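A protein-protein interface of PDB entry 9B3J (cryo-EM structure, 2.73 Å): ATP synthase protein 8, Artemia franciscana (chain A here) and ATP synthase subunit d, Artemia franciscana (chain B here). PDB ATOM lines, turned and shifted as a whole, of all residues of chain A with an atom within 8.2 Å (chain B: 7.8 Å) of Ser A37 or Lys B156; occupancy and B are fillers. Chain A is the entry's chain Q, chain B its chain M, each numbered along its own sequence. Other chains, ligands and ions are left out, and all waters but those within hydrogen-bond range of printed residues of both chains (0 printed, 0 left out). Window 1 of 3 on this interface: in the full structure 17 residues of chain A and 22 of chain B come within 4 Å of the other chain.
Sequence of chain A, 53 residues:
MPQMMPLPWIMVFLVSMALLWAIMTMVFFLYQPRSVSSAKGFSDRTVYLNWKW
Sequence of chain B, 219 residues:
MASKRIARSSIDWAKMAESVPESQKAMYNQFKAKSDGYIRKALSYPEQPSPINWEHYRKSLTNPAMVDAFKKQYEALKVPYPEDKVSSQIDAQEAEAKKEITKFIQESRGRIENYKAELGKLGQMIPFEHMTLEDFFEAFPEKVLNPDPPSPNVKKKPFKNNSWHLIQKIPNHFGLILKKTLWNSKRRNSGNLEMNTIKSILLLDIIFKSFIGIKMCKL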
ATOM      1  N   TYR A  31     -15.302 -25.401  28.251  1.00  0.00           N
ATOM      2  CA  TYR A  31     -16.307 -25.237  27.215  1.00  0.00           C
ATOM      3  C   TYR A  31     -15.776 -24.260  26.182  1.00  0.00           C
ATOM      4  O   TYR A  31     -14.905 -23.436  26.471  1.00  0.00           O
ATOM      5  CB  TYR A  31     -17.634 -24.745  27.792  1.00  0.00           C
ATOM      6  CG  TYR A  31     -17.692 -23.256  27.998  1.00  0.00           C
ATOM      7  CD1 TYR A  31     -16.920 -22.636  28.968  1.00  0.00           C
ATOM      8  CD2 TYR A  31     -18.527 -22.468  27.223  1.00  0.00           C
ATOM      9  CE1 TYR A  31     -16.974 -21.276  29.155  1.00  0.00           C
ATOM     10  CE2 TYR A  31     -18.589 -21.111  27.403  1.00  0.00           C
ATOM     11  CZ  TYR A  31     -17.810 -20.520  28.369  1.00  0.00           C
ATOM     12  OH  TYR A  31     -17.873 -19.164  28.549  1.00  0.00           O
ATOM     13  N   PRO A  33     -16.675 -21.161  23.947  1.00  0.00           N
ATOM     14  CA  PRO A  33     -17.699 -20.133  23.742  1.00  0.00           C
ATOM     15  C   PRO A  33     -17.864 -19.786  22.274  1.00  0.00           C
ATOM     16  O   PRO A  33     -17.035 -19.081  21.692  1.00  0.00           O
ATOM     17  CB  PRO A  33     -17.165 -18.949  24.554  1.00  0.00           C
ATOM     18  CG  PRO A  33     -15.695 -19.146  24.586  1.00  0.00           C
ATOM     19  CD  PRO A  33     -15.452 -20.622  24.559  1.00  0.00           C
ATOM     20  N   ARG A  34     -18.942 -20.268  21.667  1.00  0.00           N
ATOM     21  CA  ARG A  34     -19.166 -20.082  20.240  1.00  0.00           C
ATOM     22  C   ARG A  34     -19.908 -18.771  20.024  1.00  0.00           C
ATOM     23  O   ARG A  34     -21.074 -18.635  20.409  1.00  0.00           O
ATOM     24  CB  ARG A  34     -19.938 -21.258  19.655  1.00  0.00           C
ATOM     25  CG  ARG A  34     -19.086 -22.486  19.428  1.00  0.00           C
ATOM     26  CD  ARG A  34     -19.808 -23.487  18.555  1.00  0.00           C
ATOM     27  NE  ARG A  34     -19.000 -24.674  18.305  1.00  0.00           N
ATOM     28  CZ  ARG A  34     -19.337 -25.643  17.466  1.00  0.00           C
ATOM     29  NH1 ARG A  34     -20.464 -25.598  16.773  1.00  0.00           N
ATOM     30  NH2 ARG A  34     -18.523 -26.684  17.316  1.00  0.00           N
ATOM     31  N   SER A  35     -19.227 -17.805  19.412  1.00  0.00           N
ATOM     32  CA  SER A  35     -19.831 -16.520  19.068  1.00  0.00           C
ATOM     33  C   SER A  35     -20.409 -16.594  17.656  1.00  0.00           C
ATOM     34  O   SER A  35     -19.888 -16.022  16.699  1.00  0.00           O
ATOM     35  CB  SER A  35     -18.809 -15.400  19.192  1.00  0.00           C
ATOM     36  OG  SER A  35     -19.336 -14.194  18.675  1.00  0.00           O
ATOM     37  N   VAL A  36     -21.521 -17.318  17.544  1.00  0.00           N
ATOM     38  CA  VAL A  36     -22.199 -17.480  16.263  1.00  0.00           C
ATOM     39  C   VAL A  36     -23.509 -16.705  16.322  1.00  0.00           C
ATOM     40  O   VAL A  36     -24.504 -17.082  15.692  1.00  0.00           O
ATOM     41  CB  VAL A  36     -22.434 -18.964  15.923  1.00  0.00           C
ATOM     42  CG1 VAL A  36     -22.413 -19.180  14.413  1.00  0.00           C
ATOM     43  CG2 VAL A  36     -21.390 -19.835  16.588  1.00  0.00           C
ATOM     44  N   SER A  37     -23.520 -15.624  17.094  1.00  0.00           N
ATOM     45  CA  SER A  37     -24.691 -14.756  17.184  1.00  0.00           C
ATOM     46  C   SER A  37     -24.787 -13.934  15.906  1.00  0.00           C
ATOM     47  O   SER A  37     -24.136 -12.897  15.768  1.00  0.00           O
ATOM     48  CB  SER A  37     -24.595 -13.860  18.413  1.00  0.00           C
ATOM     49  OG  SER A  37     -25.735 -13.023  18.517  1.00  0.00           O
ATOM     50  N   SER A  38     -25.597 -14.398  14.961  1.00  0.00           N
ATOM     51  CA  SER A  38     -25.747 -13.698  13.693  1.00  0.00           C
ATOM     52  C   SER A  38     -26.534 -12.406  13.878  1.00  0.00           C
ATOM     53  O   SER A  38     -27.459 -12.330  14.691  1.00  0.00           O
ATOM     54  CB  SER A  38     -26.440 -14.597  12.671  1.00  0.00           C
ATOM     55  OG  SER A  38     -27.717 -15.003  13.132  1.00  0.00           O
ATOM     56  N   ALA A  39     -26.158 -11.384  13.112  1.00  0.00           N
ATOM     57  CA  ALA A  39     -26.819 -10.081  13.137  1.00  0.00           C
ATOM     58  C   ALA A  39     -27.732  -9.889  11.934  1.00  0.00           C
ATOM     59  O   ALA A  39     -27.819  -8.794  11.373  1.00  0.00           O
ATOM     60  CB  ALA A  39     -25.785  -8.963  13.210  1.00  0.00           C
ATOM     61  N   LYS A  40     -28.415 -10.952  11.506  1.00  0.00           N
ATOM     62  CA  LYS A  40     -29.339 -10.850  10.385  1.00  0.00           C
ATOM     63  C   LYS A  40     -30.641 -10.153  10.764  1.00  0.00           C
ATOM     64  O   LYS A  40     -31.353  -9.666   9.875  1.00  0.00           O
ATOM     65  CB  LYS A  40     -29.633 -12.244   9.824  1.00  0.00           C
ATOM     66  CG  LYS A  40     -30.103 -12.258   8.377  1.00  0.00           C
ATOM     67  CD  LYS A  40     -30.429 -13.667   7.918  1.00  0.00           C
ATOM     68  CE  LYS A  40     -29.224 -14.583   8.059  1.00  0.00           C
ATOM     69  NZ  LYS A  40     -29.533 -15.978   7.636  1.00  0.00           N
ATOM     70  N   PHE A  42     -30.951  -7.293  12.179  1.00  0.00           N
ATOM     71  CA  PHE A  42     -30.816  -5.887  11.815  1.00  0.00           C
ATOM     72  C   PHE A  42     -31.124  -5.629  10.347  1.00  0.00           C
ATOM     73  O   PHE A  42     -31.324  -4.469   9.969  1.00  0.00           O
ATOM     74  CB  PHE A  42     -29.409  -5.390  12.140  1.00  0.00           C
ATOM     75  CG  PHE A  42     -29.162  -5.191  13.605  1.00  0.00           C
ATOM     76  CD1 PHE A  42     -29.456  -3.981  14.210  1.00  0.00           C
ATOM     77  CD2 PHE A  42     -28.632  -6.212  14.377  1.00  0.00           C
ATOM     78  CE1 PHE A  42     -29.230  -3.791  15.558  1.00  0.00           C
ATOM     79  CE2 PHE A  42     -28.404  -6.029  15.728  1.00  0.00           C
ATOM     80  CZ  PHE A  42     -28.702  -4.816  16.318  1.00  0.00           C
ATOM     81  N   PHE B 140     -16.520  -9.567  24.276  1.00  0.00           N
ATOM     82  CA  PHE B 140     -17.878 -10.101  24.342  1.00  0.00           C
ATOM     83  C   PHE B 140     -18.229 -10.269  25.812  1.00  0.00           C
ATOM     84  O   PHE B 140     -18.014 -11.336  26.398  1.00  0.00           O
ATOM     85  CB  PHE B 140     -17.997 -11.411  23.579  1.00  0.00           C
ATOM     86  CG  PHE B 140     -17.779 -11.265  22.109  1.00  0.00           C
ATOM     87  CD1 PHE B 140     -16.504 -11.286  21.578  1.00  0.00           C
ATOM     88  CD2 PHE B 140     -18.851 -11.104  21.256  1.00  0.00           C
ATOM     89  CE1 PHE B 140     -16.302 -11.150  20.227  1.00  0.00           C
ATOM     90  CE2 PHE B 140     -18.656 -10.968  19.903  1.00  0.00           C
ATOM     91  CZ  PHE B 140     -17.380 -10.990  19.387  1.00  0.00           C
ATOM     92  N   GLU B 142     -20.581 -10.939  27.760  1.00  0.00           N
ATOM     93  CA  GLU B 142     -21.552 -11.847  28.366  1.00  0.00           C
ATOM     94  C   GLU B 142     -20.883 -12.755  29.393  1.00  0.00           C
ATOM     95  O   GLU B 142     -21.396 -12.924  30.506  1.00  0.00           O
ATOM     96  CB  GLU B 142     -22.260 -12.667  27.287  1.00  0.00           C
ATOM     97  CG  GLU B 142     -21.503 -12.782  25.981  1.00  0.00           C
ATOM     98  CD  GLU B 142     -20.475 -13.888  25.988  1.00  0.00           C
ATOM     99  OE1 GLU B 142     -20.437 -14.660  26.968  1.00  0.00           O
ATOM    100  OE2 GLU B 142     -19.711 -13.986  25.008  1.00  0.00           O
ATOM    101  N   ASN B 153     -21.381 -27.278  30.386  1.00  0.00           N
ATOM    102  CA  ASN B 153     -21.319 -26.800  29.012  1.00  0.00           C
ATOM    103  C   ASN B 153     -22.075 -25.483  29.015  1.00  0.00           C
ATOM    104  O   ASN B 153     -23.292 -25.456  28.836  1.00  0.00           O
ATOM    105  CB  ASN B 153     -21.933 -27.790  28.051  1.00  0.00           C
ATOM    106  CG  ASN B 153     -23.079 -28.561  28.667  1.00  0.00           C
ATOM    107  OD1 ASN B 153     -23.042 -29.787  28.746  1.00  0.00           O
ATOM    108  ND2 ASN B 153     -24.103 -27.848  29.114  1.00  0.00           N
ATOM    109  N   VAL B 154     -21.351 -24.391  29.227  1.00  0.00           N
ATOM    110  CA  VAL B 154     -22.007 -23.103  29.381  1.00  0.00           C
ATOM    111  C   VAL B 154     -22.462 -22.677  27.995  1.00  0.00           C
ATOM    112  O   VAL B 154     -21.713 -22.047  27.243  1.00  0.00           O
ATOM    113  CB  VAL B 154     -21.068 -22.065  30.019  1.00  0.00           C
ATOM    114  CG1 VAL B 154     -21.873 -20.995  30.714  1.00  0.00           C
ATOM    115  CG2 VAL B 154     -20.125 -22.728  30.994  1.00  0.00           C
ATOM    116  N   LYS B 155     -23.699 -23.012  27.663  1.00  0.00           N
ATOM    117  CA  LYS B 155     -24.221 -22.918  26.314  1.00  0.00           C
ATOM    118  C   LYS B 155     -25.307 -21.849  26.262  1.00  0.00           C
ATOM    119  O   LYS B 155     -25.551 -21.131  27.238  1.00  0.00           O
ATOM    120  CB  LYS B 155     -24.744 -24.284  25.869  1.00  0.00           C
ATOM    121  CG  LYS B 155     -24.448 -24.637  24.430  1.00  0.00           C
ATOM    122  CD  LYS B 155     -25.466 -25.630  23.903  1.00  0.00           C
ATOM    123  CE  LYS B 155     -25.525 -26.873  24.765  1.00  0.00           C
ATOM    124  NZ  LYS B 155     -24.229 -27.596  24.756  1.00  0.00           N
ATOM    125  N   LYS B 156     -25.963 -21.737  25.110  1.00  0.00           N
ATOM    126  CA  LYS B 156     -27.070 -20.808  24.959  1.00  0.00           C
ATOM    127  C   LYS B 156     -28.406 -21.398  25.388  1.00  0.00           C
ATOM    128  O   LYS B 156     -29.365 -20.642  25.567  1.00  0.00           O
ATOM    129  CB  LYS B 156     -27.153 -20.318  23.508  1.00  0.00           C
ATOM    130  CG  LYS B 156     -25.949 -19.490  23.081  1.00  0.00           C
ATOM    131  CD  LYS B 156     -26.114 -18.921  21.680  1.00  0.00           C
ATOM    132  CE  LYS B 156     -24.919 -18.058  21.293  1.00  0.00           C
ATOM    133  NZ  LYS B 156     -25.050 -17.481  19.926  1.00  0.00           N
ATOM    134  N   LYS B 157     -28.499 -22.716  25.560  1.00  0.00           N
ATOM    135  CA  LYS B 157     -29.717 -23.265  26.151  1.00  0.00           C
ATOM    136  C   LYS B 157     -29.527 -24.462  27.088  1.00  0.00           C
ATOM    137  O   LYS B 157     -30.213 -25.476  26.903  1.00  0.00           O
ATOM    138  CB  LYS B 157     -30.678 -23.661  25.028  1.00  0.00           C
ATOM    139  CG  LYS B 157     -30.021 -24.408  23.872  1.00  0.00           C
ATOM    140  CD  LYS B 157     -29.899 -23.535  22.634  1.00  0.00           C
ATOM    141  CE  LYS B 157     -31.265 -23.159  22.087  1.00  0.00           C
ATOM    142  NZ  LYS B 157     -32.044 -24.356  21.670  1.00  0.00           N
ATOM    143  N   PRO B 158     -28.643 -24.417  28.118  1.00  0.00           N
ATOM    144  CA  PRO B 158     -28.631 -25.530  29.075  1.00  0.00           C
ATOM    145  C   PRO B 158     -29.391 -25.254  30.367  1.00  0.00           C
ATOM    146  O   PRO B 158     -29.576 -26.169  31.177  1.00  0.00           O
ATOM    147  CB  PRO B 158     -27.136 -25.732  29.340  1.00  0.00           C
ATOM    148  CG  PRO B 158     -26.522 -24.383  29.100  1.00  0.00           C
ATOM    149  CD  PRO B 158     -27.527 -23.499  28.412  1.00  0.00           C
ATOM    150  N   PHE B 159     -29.839 -24.020  30.580  1.00  0.00           N
ATOM    151  CA  PHE B 159     -30.500 -23.630  31.813  1.00  0.00           C
ATOM    152  C   PHE B 159     -31.888 -23.082  31.516  1.00  0.00           C
ATOM    153  O   PHE B 159     -32.156 -22.577  30.422  1.00  0.00           O
ATOM    154  CB  PHE B 159     -29.685 -22.583  32.590  1.00  0.00           C
ATOM    155  CG  PHE B 159     -29.183 -21.448  31.747  1.00  0.00           C
ATOM    156  CD1 PHE B 159     -29.994 -20.364  31.455  1.00  0.00           C
ATOM    157  CD2 PHE B 159     -27.887 -21.454  31.269  1.00  0.00           C
ATOM    158  CE1 PHE B 159     -29.528 -19.321  30.688  1.00  0.00           C
ATOM    159  CE2 PHE B 159     -27.416 -20.414  30.500  1.00  0.00           C
ATOM    160  CZ  PHE B 159     -28.237 -19.345  30.210  1.00  0.00           C
ATOM    161  N   ASN B 161     -35.591 -22.842  30.482  1.00  0.00           N
ATOM    162  CA  ASN B 161     -36.251 -23.470  29.331  1.00  0.00           C
ATOM    163  C   ASN B 161     -37.170 -24.615  29.758  1.00  0.00           C
ATOM    164  O   ASN B 161     -37.213 -25.673  29.126  1.00  0.00           O
ATOM    165  CB  ASN B 161     -35.225 -23.943  28.297  1.00  0.00           C
ATOM    166  CG  ASN B 161     -34.279 -22.839  27.874  1.00  0.00           C
ATOM    167  OD1 ASN B 161     -34.150 -21.823  28.556  1.00  0.00           O
ATOM    168  ND2 ASN B 161     -33.615 -23.029  26.740  1.00  0.00           N
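Of the printed residues of chain B, Tyr A31 touches Val B154. Of the printed residues of chain B, Arg A34 touches Lys B156. Printed residues of chain B within 4 Å of Ser A35: Phe B140 (3.5 Å). Printed residues of chain B within 4 Å of Val A36: Lys B156. Of chain B, only Lys B156 comes within 4 Å of Ser A37. Of the printed residues of chain A, Val B154 touches Tyr A31 (3.2 Å). Printed residues of chain A within 4 Å of Lys B156: Arg A34 (3.99 Å), Val A36 (3.996 Å) and Ser A37 (3.7 Å). The nearest residue of chain B that does not touch Ser A37 is Phe B140 (6.8 Å). The nearest printed residue of chain A that does not touch Lys B156 is Ser A35 (5.2 Å).
O of Val B154 touches CD2 of Tyr A31, at 3.2 Å. Arg A34 touches Lys B156 (O to CE, 3.99 Å). CE2 of Phe B140 touches OG of Ser A35, at 3.5 Å. C of Val A36 touches NZ of Lys B156 (3.996 Å). N of Ser A37 touches NZ of Lys B156 (3.7 Å).
Of the 10 printed residues of chain A, 5 touch a printed residue of chain B. Printed residues of chain A that touch a printed residue of chain B: Tyr A31, Arg A34, Ser A35, Val A36 and Ser A37. Of the 10 printed residues of chain B, 3 touch a printed residue of chain A. Printed residues of chain B that touch a printed residue of chain A: Phe B140, Val B154 and Lys B156. Hydrophobic or aromatic side chains of chain B that line the printed part of chain A: Phe B140 and Val B154. Among the printed residues, 5 pairs touch across the chains. Among the printed residues, no Asp or Glu carboxylate lies within 4 Å of a Lys or Arg side-chain nitrogen of the other chain.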
